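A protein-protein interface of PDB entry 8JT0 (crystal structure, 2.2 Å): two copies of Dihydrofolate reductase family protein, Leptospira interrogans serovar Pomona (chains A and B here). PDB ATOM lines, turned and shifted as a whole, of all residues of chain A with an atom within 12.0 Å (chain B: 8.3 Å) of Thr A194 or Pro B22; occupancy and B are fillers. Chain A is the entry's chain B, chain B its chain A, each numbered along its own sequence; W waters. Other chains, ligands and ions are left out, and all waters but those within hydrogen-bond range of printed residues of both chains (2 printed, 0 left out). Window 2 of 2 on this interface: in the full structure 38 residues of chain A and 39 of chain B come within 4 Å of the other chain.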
ATOM      1  N   VAL A 190      16.671  27.091  -2.818  1.00  0.00           N
ATOM      2  CA  VAL A 190      16.770  25.640  -2.489  1.00  0.00           C
ATOM      3  C   VAL A 190      17.981  25.040  -3.205  1.00  0.00           C
ATOM      4  O   VAL A 190      18.186  25.366  -4.385  1.00  0.00           O
ATOM      5  CB  VAL A 190      15.472  24.897  -2.859  1.00  0.00           C
ATOM      6  CG1 VAL A 190      15.558  23.412  -2.553  1.00  0.00           C
ATOM      7  CG2 VAL A 190      14.262  25.510  -2.177  1.00  0.00           C
ATOM      8  N   LYS A 191      18.732  24.189  -2.514  1.00  0.00           N
ATOM      9  CA  LYS A 191      19.921  23.560  -3.066  1.00  0.00           C
ATOM     10  C   LYS A 191      19.667  22.076  -3.287  1.00  0.00           C
ATOM     11  O   LYS A 191      19.094  21.404  -2.423  1.00  0.00           O
ATOM     12  CB  LYS A 191      21.121  23.741  -2.127  1.00  0.00           C
ATOM     13  CG  LYS A 191      21.689  25.154  -2.090  1.00  0.00           C
ATOM     14  CD  LYS A 191      21.705  25.764  -3.476  1.00  0.00           C
ATOM     15  CE  LYS A 191      22.389  27.124  -3.480  1.00  0.00           C
ATOM     16  NZ  LYS A 191      21.883  27.967  -4.598  1.00  0.00           N
ATOM     17  N   THR A 192      20.099  21.569  -4.448  1.00  0.00           N
ATOM     18  CA  THR A 192      20.048  20.143  -4.760  1.00  0.00           C
ATOM     19  C   THR A 192      21.417  19.670  -5.215  1.00  0.00           C
ATOM     20  O   THR A 192      22.112  20.364  -5.963  1.00  0.00           O
ATOM     21  CB  THR A 192      19.027  19.802  -5.872  1.00  0.00           C
ATOM     22  OG1 THR A 192      19.383  20.476  -7.080  1.00  0.00           O
ATOM     23  CG2 THR A 192      17.609  20.198  -5.464  1.00  0.00           C
ATOM     24  N   GLY A 193      21.791  18.485  -4.769  1.00  0.00           N
ATOM     25  CA  GLY A 193      22.927  17.785  -5.322  1.00  0.00           C
ATOM     26  C   GLY A 193      22.571  16.340  -5.606  1.00  0.00           C
ATOM     27  O   GLY A 193      21.405  15.995  -5.833  1.00  0.00           O
ATOM     28  N   THR A 194      23.592  15.494  -5.591  1.00  0.00           N
ATOM     29  CA  THR A 194      23.448  14.050  -5.691  1.00  0.00           C
ATOM     30  C   THR A 194      24.163  13.451  -4.498  1.00  0.00           C
ATOM     31  O   THR A 194      25.341  13.739  -4.276  1.00  0.00           O
ATOM     32  CB  THR A 194      24.039  13.524  -7.001  1.00  0.00           C
ATOM     33  OG1 THR A 194      23.531  14.290  -8.099  1.00  0.00           O
ATOM     34  CG2 THR A 194      23.691  12.065  -7.202  1.00  0.00           C
ATOM     35  N   VAL A 195      23.454  12.644  -3.722  1.00  0.00           N
ATOM     36  CA  VAL A 195      24.046  12.068  -2.522  1.00  0.00           C
ATOM     37  C   VAL A 195      25.030  10.962  -2.889  1.00  0.00           C
ATOM     38  O   VAL A 195      24.690  10.032  -3.618  1.00  0.00           O
ATOM     39  CB  VAL A 195      22.962  11.550  -1.558  1.00  0.00           C
ATOM     40  CG1 VAL A 195      22.148  12.719  -1.025  1.00  0.00           C
ATOM     41  CG2 VAL A 195      22.043  10.552  -2.251  1.00  0.00           C
ATOM     42  N   GLN B  17       9.403  13.304  -2.077  1.00  0.00           N
ATOM     43  CA  GLN B  17       9.766  12.841  -3.410  1.00  0.00           C
ATOM     44  C   GLN B  17      11.236  13.137  -3.706  1.00  0.00           C
ATOM     45  O   GLN B  17      11.699  14.272  -3.551  1.00  0.00           O
ATOM     46  CB  GLN B  17       8.865  13.504  -4.452  1.00  0.00           C
ATOM     47  CG  GLN B  17       9.287  13.280  -5.893  1.00  0.00           C
ATOM     48  CD  GLN B  17       8.157  13.601  -6.848  1.00  0.00           C
ATOM     49  OE1 GLN B  17       7.041  13.881  -6.407  1.00  0.00           O
ATOM     50  NE2 GLN B  17       8.426  13.569  -8.152  1.00  0.00           N
ATOM     51  N   ALA B  18      11.974  12.094  -4.114  1.00  0.00           N
ATOM     52  CA  ALA B  18      13.319  12.201  -4.675  1.00  0.00           C
ATOM     53  C   ALA B  18      14.309  12.910  -3.765  1.00  0.00           C
ATOM     54  O   ALA B  18      14.883  13.938  -4.153  1.00  0.00           O
ATOM     55  CB  ALA B  18      13.256  12.923  -6.019  1.00  0.00           C
ATOM     56  N   PRO B  19      14.557  12.400  -2.557  1.00  0.00           N
ATOM     57  CA  PRO B  19      15.561  13.057  -1.711  1.00  0.00           C
ATOM     58  C   PRO B  19      16.956  13.051  -2.315  1.00  0.00           C
ATOM     59  O   PRO B  19      17.695  14.037  -2.162  1.00  0.00           O
ATOM     60  CB  PRO B  19      15.498  12.252  -0.404  1.00  0.00           C
ATOM     61  CG  PRO B  19      14.942  10.945  -0.794  1.00  0.00           C
ATOM     62  CD  PRO B  19      13.985  11.212  -1.911  1.00  0.00           C
ATOM     63  N   GLY B  20      17.326  11.980  -3.026  1.00  0.00           N
ATOM     64  CA  GLY B  20      18.730  11.685  -3.265  1.00  0.00           C
ATOM     65  C   GLY B  20      19.353  12.265  -4.514  1.00  0.00           C
ATOM     66  O   GLY B  20      20.577  12.417  -4.589  1.00  0.00           O
ATOM     67  N   GLY B  21      18.539  12.610  -5.499  1.00  0.00           N
ATOM     68  CA  GLY B  21      19.096  13.013  -6.759  1.00  0.00           C
ATOM     69  C   GLY B  21      18.118  13.659  -7.697  1.00  0.00           C
ATOM     70  O   GLY B  21      16.906  13.418  -7.676  1.00  0.00           O
ATOM     71  N   PRO B  22      18.663  14.469  -8.583  1.00  0.00           N
ATOM     72  CA  PRO B  22      17.834  15.193  -9.559  1.00  0.00           C
ATOM     73  C   PRO B  22      16.894  14.299 -10.367  1.00  0.00           C
ATOM     74  O   PRO B  22      15.825  14.767 -10.795  1.00  0.00           O
ATOM     75  CB  PRO B  22      18.873  15.856 -10.481  1.00  0.00           C
ATOM     76  CG  PRO B  22      20.218  15.663  -9.821  1.00  0.00           C
ATOM     77  CD  PRO B  22      20.111  14.558  -8.846  1.00  0.00           C
ATOM     78  N   GLU B  23      17.253  13.034 -10.593  1.00  0.00           N
ATOM     79  CA  GLU B  23      16.456  12.152 -11.439  1.00  0.00           C
ATOM     80  C   GLU B  23      15.858  10.977 -10.684  1.00  0.00           C
ATOM     81  O   GLU B  23      15.210  10.124 -11.308  1.00  0.00           O
ATOM     82  CB  GLU B  23      17.301  11.623 -12.599  1.00  0.00           C
ATOM     83  CG  GLU B  23      17.828  12.692 -13.506  1.00  0.00           C
ATOM     84  CD  GLU B  23      18.442  12.090 -14.762  1.00  0.00           C
ATOM     85  OE1 GLU B  23      19.301  11.168 -14.638  1.00  0.00           O
ATOM     86  OE2 GLU B  23      18.055  12.533 -15.868  1.00  0.00           O
ATOM     87  N   GLU B  24      16.023  10.940  -9.367  1.00  0.00           N
ATOM     88  CA  GLU B  24      15.451   9.840  -8.549  1.00  0.00           C
ATOM     89  C   GLU B  24      13.955   9.669  -8.831  1.00  0.00           C
ATOM     90  O   GLU B  24      13.521   8.518  -8.909  1.00  0.00           O
ATOM     91  CB  GLU B  24      15.701  10.083  -7.064  1.00  0.00           C
ATOM     92  CG  GLU B  24      15.323   8.908  -6.190  1.00  0.00           C
ATOM     93  CD  GLU B  24      15.416   9.197  -4.704  1.00  0.00           C
ATOM     94  OE1 GLU B  24      16.330   9.926  -4.307  1.00  0.00           O
ATOM     95  OE2 GLU B  24      14.574   8.688  -3.954  1.00  0.00           O
ATOM     96  N   ASP B  25      13.200  10.761  -8.953  1.00  0.00           N
ATOM     97  CA  ASP B  25      11.749  10.698  -9.274  1.00  0.00           C
ATOM     98  C   ASP B  25      11.348  11.992  -9.976  1.00  0.00           C
ATOM     99  O   ASP B  25      11.252  13.016  -9.301  1.00  0.00           O
ATOM    100  CB  ASP B  25      10.881  10.440  -8.045  1.00  0.00           C
ATOM    101  CG  ASP B  25       9.415  10.206  -8.353  1.00  0.00           C
ATOM    102  OD1 ASP B  25       9.077  10.104  -9.539  1.00  0.00           O
ATOM    103  OD2 ASP B  25       8.630  10.122  -7.399  1.00  0.00           O
ATOM    104  N   THR B  26      11.089  11.914 -11.272  1.00  0.00           N
ATOM    105  CA  THR B  26      10.777  13.119 -12.073  1.00  0.00           C
ATOM    106  C   THR B  26       9.266  13.235 -12.258  1.00  0.00           C
ATOM    107  O   THR B  26       8.846  14.040 -13.090  1.00  0.00           O
ATOM    108  CB  THR B  26      11.526  13.047 -13.408  1.00  0.00           C
ATOM    109  OG1 THR B  26      11.229  11.795 -14.023  1.00  0.00           O
ATOM    110  CG2 THR B  26      13.021  13.201 -13.241  1.00  0.00           C
ATOM    111  N   SER B  27       8.495  12.436 -11.525  1.00  0.00           N
ATOM    112  CA  SER B  27       7.014  12.503 -11.597  1.00  0.00           C
ATOM    113  C   SER B  27       6.552  13.960 -11.484  1.00  0.00           C
ATOM    114  O   SER B  27       7.032  14.655 -10.581  1.00  0.00           O
ATOM    115  CB  SER B  27       6.391  11.655 -10.529  1.00  0.00           C
ATOM    116  OG  SER B  27       6.866  10.324 -10.597  1.00  0.00           O
ATOM    117  N   GLY B  29       7.283  16.390 -13.306  1.00  0.00           N
ATOM    118  CA  GLY B  29       8.303  17.363 -13.650  1.00  0.00           C
ATOM    119  C   GLY B  29       9.049  17.926 -12.465  1.00  0.00           C
ATOM    120  O   GLY B  29       9.712  18.963 -12.602  1.00  0.00           O
ATOM    121  N   PHE B  30       8.981  17.242 -11.312  1.00  0.00           N
ATOM    122  CA  PHE B  30       9.601  17.643 -10.056  1.00  0.00           C
ATOM    123  C   PHE B  30      11.040  18.101 -10.255  1.00  0.00           C
ATOM    124  O   PHE B  30      11.928  17.307 -10.609  1.00  0.00           O
ATOM    125  CB  PHE B  30       9.526  16.474  -9.067  1.00  0.00           C
ATOM    126  CG  PHE B  30      10.021  16.780  -7.677  1.00  0.00           C
ATOM    127  CD1 PHE B  30       9.299  17.598  -6.807  1.00  0.00           C
ATOM    128  CD2 PHE B  30      11.186  16.196  -7.208  1.00  0.00           C
ATOM    129  CE1 PHE B  30       9.760  17.842  -5.495  1.00  0.00           C
ATOM    130  CE2 PHE B  30      11.656  16.444  -5.903  1.00  0.00           C
ATOM    131  CZ  PHE B  30      10.936  17.278  -5.055  1.00  0.00           C
ATOM    132  N   LYS B  31      11.273  19.384  -9.983  1.00  0.00           N
ATOM    133  CA  LYS B  31      12.539  20.040 -10.258  1.00  0.00           C
ATOM    134  C   LYS B  31      13.545  19.918  -9.127  1.00  0.00           C
ATOM    135  O   LYS B  31      14.719  20.241  -9.334  1.00  0.00           O
ATOM    136  CB  LYS B  31      12.300  21.517 -10.582  1.00  0.00           C
ATOM    137  CG  LYS B  31      11.435  21.685 -11.815  1.00  0.00           C
ATOM    138  CD  LYS B  31      11.286  23.125 -12.258  1.00  0.00           C
ATOM    139  CE  LYS B  31      10.574  23.193 -13.611  1.00  0.00           C
ATOM    140  NZ  LYS B  31      10.613  24.564 -14.225  1.00  0.00           N
ATOM    141  N   TYR B  32      13.150  19.413  -7.964  1.00  0.00           N
ATOM    142  CA  TYR B  32      13.979  19.556  -6.773  1.00  0.00           C
ATOM    143  C   TYR B  32      14.590  18.244  -6.296  1.00  0.00           C
ATOM    144  O   TYR B  32      15.027  18.153  -5.137  1.00  0.00           O
ATOM    145  CB  TYR B  32      13.170  20.233  -5.655  1.00  0.00           C
ATOM    146  CG  TYR B  32      12.787  21.641  -6.050  1.00  0.00           C
ATOM    147  CD1 TYR B  32      13.721  22.665  -5.992  1.00  0.00           C
ATOM    148  CD2 TYR B  32      11.522  21.934  -6.537  1.00  0.00           C
ATOM    149  CE1 TYR B  32      13.405  23.942  -6.380  1.00  0.00           C
ATOM    150  CE2 TYR B  32      11.191  23.220  -6.934  1.00  0.00           C
ATOM    151  CZ  TYR B  32      12.141  24.220  -6.845  1.00  0.00           C
ATOM    152  OH  TYR B  32      11.845  25.504  -7.237  1.00  0.00           O
ATOM    153  N   GLY B  33      14.678  17.241  -7.176  1.00  0.00           N
ATOM    154  CA  GLY B  33      15.332  16.008  -6.798  1.00  0.00           C
ATOM    155  C   GLY B  33      16.721  16.303  -6.270  1.00  0.00           C
ATOM    156  O   GLY B  33      17.418  17.176  -6.796  1.00  0.00           O
ATOM    157  N   GLY B  34      17.112  15.623  -5.203  1.00  0.00           N
ATOM    158  CA  GLY B  34      18.382  15.903  -4.579  1.00  0.00           C
ATOM    159  C   GLY B  34      18.352  16.931  -3.464  1.00  0.00           C
ATOM    160  O   GLY B  34      19.425  17.283  -2.948  1.00  0.00           O
ATOM    161  N   TRP B  35      17.160  17.397  -3.052  1.00  0.00           N
ATOM    162  CA  TRP B  35      17.052  18.442  -2.030  1.00  0.00           C
ATOM    163  C   TRP B  35      17.660  18.035  -0.694  1.00  0.00           C
ATOM    164  O   TRP B  35      17.971  18.907   0.122  1.00  0.00           O
ATOM    165  CB  TRP B  35      15.588  18.834  -1.814  1.00  0.00           C
ATOM    166  CG  TRP B  35      14.693  17.678  -1.498  1.00  0.00           C
ATOM    167  CD1 TRP B  35      13.970  16.942  -2.392  1.00  0.00           C
ATOM    168  CD2 TRP B  35      14.424  17.116  -0.201  1.00  0.00           C
ATOM    169  NE1 TRP B  35      13.258  15.959  -1.734  1.00  0.00           N
ATOM    170  CE2 TRP B  35      13.515  16.048  -0.390  1.00  0.00           C
ATOM    171  CE3 TRP B  35      14.838  17.426   1.098  1.00  0.00           C
ATOM    172  CZ2 TRP B  35      13.021  15.282   0.672  1.00  0.00           C
ATOM    173  CZ3 TRP B  35      14.347  16.661   2.159  1.00  0.00           C
ATOM    174  CH2 TRP B  35      13.450  15.602   1.938  1.00  0.00           C
ATOM    175  N   THR B  36      17.830  16.741  -0.448  1.00  0.00           N
ATOM    176  CA  THR B  36      18.475  16.273   0.775  1.00  0.00           C
ATOM    177  C   THR B  36      20.002  16.378   0.721  1.00  0.00           C
ATOM    178  O   THR B  36      20.649  16.365   1.776  1.00  0.00           O
ATOM    179  CB  THR B  36      18.053  14.825   1.024  1.00  0.00           C
ATOM    180  OG1 THR B  36      17.708  14.642   2.399  1.00  0.00           O
ATOM    181  CG2 THR B  36      19.161  13.855   0.662  1.00  0.00           C
ATOM    182  N   ALA B  37      20.596  16.489  -0.475  1.00  0.00           N
ATOM    183  CA  ALA B  37      22.055  16.410  -0.589  1.00  0.00           C
ATOM    184  C   ALA B  37      22.795  17.487   0.200  1.00  0.00           C
ATOM    185  O   ALA B  37      23.770  17.147   0.894  1.00  0.00           O
ATOM    186  CB  ALA B  37      22.460  16.427  -2.069  1.00  0.00           C
ATOM    187  N   PRO B  38      22.406  18.776   0.162  1.00  0.00           N
ATOM    188  CA  PRO B  38      23.166  19.795   0.909  1.00  0.00           C
ATOM    189  C   PRO B  38      23.188  19.665   2.429  1.00  0.00           C
ATOM    190  O   PRO B  38      23.809  20.507   3.075  1.00  0.00           O
ATOM    191  CB  PRO B  38      22.487  21.114   0.508  1.00  0.00           C
ATOM    192  CG  PRO B  38      21.238  20.738  -0.196  1.00  0.00           C
ATOM    193  CD  PRO B  38      21.430  19.389  -0.761  1.00  0.00           C
ATOM    194  N   GLU B  40      24.071  16.784   4.266  1.00  0.00           N
ATOM    195  CA  GLU B  40      24.782  15.547   4.565  1.00  0.00           C
ATOM    196  C   GLU B  40      26.085  15.868   5.298  1.00  0.00           C
ATOM    197  O   GLU B  40      26.902  16.646   4.793  1.00  0.00           O
ATOM    198  CB  GLU B  40      25.056  14.811   3.253  1.00  0.00           C
ATOM    199  CG  GLU B  40      25.326  13.326   3.335  1.00  0.00           C
ATOM    200  CD  GLU B  40      25.881  12.790   2.017  1.00  0.00           C
ATOM    201  OE1 GLU B  40      25.833  13.530   1.002  1.00  0.00           O
ATOM    202  OE2 GLU B  40      26.382  11.645   1.998  1.00  0.00           O
HETATM  203  O   HOH W   1      17.344  19.092  -8.842  1.00  0.00           O
HETATM  204  O   HOH W   2      17.801  21.411  -0.363  1.00  0.00           O
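Of the printed residues of chain A, Pro B22 touches Gly A193 (3.6 Å) and Thr A194 (3.5 Å).
Gly A193 touches just these residues of chain B: Gly B20, Gly B21, Pro B22, Gly B34 and Ala B37.
Val A195 touches three residues of chain B.
Glu B23 touches none of the printed residues of chain A.
Gly B34 touches just these residues of chain A: Thr A192 and Gly A193.
Of the printed residues of chain A, Ala B37 touches Gly A193 (3.5 Å), Thr A194 (3.8 Å) and Val A195 (3.7 Å).
Printed residues of chain B within 4 Å of Thr A192: Tyr B32, Gly B33, Gly B34 and Trp B35.
Of the printed residues of chain B, Val A190 touches Tyr B32 (3.97 Å).
Printed residues of chain A within 4 Å of Trp B35: Lys A191 (3.6 Å) and Thr A192 (3.7 Å).
Ser B27 touches none of the printed residues of chain A.
Gln B17 touches none of the printed residues of chain A.
The nearest residue of chain B that does not touch Thr A194 is Gly B21 (4.6 Å).
The nearest residue of chain A that does not touch Pro B22 is Thr A192 (5.6 Å).
The nearest printed residue of chain A that does not touch Tyr B32 is Lys A191 (5.9 Å).
Tyr B32 touches Val A190.
Thr A192 touches Gly B33.
Thr A192 touches Trp B35.
Gly B21 touches Gly A193.
Gly A193 touches Pro B22 (O to CD, 3.6 Å).
Thr A194 touches Gly B20 (CA to O, 3.5 Å).
Thr A194 touches Pro B22 (OG1 to CD, 3.5 Å).
CB of Ala B37 touches N of Thr A194, at 3.8 Å.
Val A195 touches Thr B36 (CG1 to CG2, 3.6 Å).
Val A195 touches Ala B37.
No position is printed for both chains.
Hydrophobic or aromatic side chains of chain B within 4 Å of the printed part of chain A: Pro B22, Tyr B32, Ala B37 and Pro B38.
Hydrophobic or aromatic side chains of chain A within 4 Å of the printed part of chain B: Val A190 and Val A195.
Among the printed residues, 18 pairs touch across the chains.
Water W2 bridges O of Lys A191 (2.4 Å) and O of Trp B35 (2.6 Å).
Water W1 lies within hydrogen-bond range of O of Gly B33 (2.8 Å), O of Lys B31 (2.9 Å) and OG1 of Thr A192 (3.0 Å).
O of Gln B17 is in hydrogen-bond range of NE1 of Trp B35, at 2.9 Å.
The backbone NH of Gly B34 sits at hydrogen-bond distance from the backbone carbonyl oxygen of Ala B18, 3.0 Å away.
The backbone carbonyl oxygen (O) of Pro B19 sits close to the backbone NH (N) of Gly B34.
N of Thr B36 sits close to O of Pro B19 (3.2 Å).
The backbone NH (N) of Gly B20 lies within hydrogen-bond range of the side-chain carboxylate (OE1) of Glu B24 (2.6 Å).
The backbone carbonyl oxygen (O) of Gly B21 is in hydrogen-bond range of the backbone NH (N) of Gly B34.
O of Gly B20 lies within hydrogen-bond range of N of Val A195 (3.0 Å).
N of Gly A193 sits at hydrogen-bond distance from O of Gly B34.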
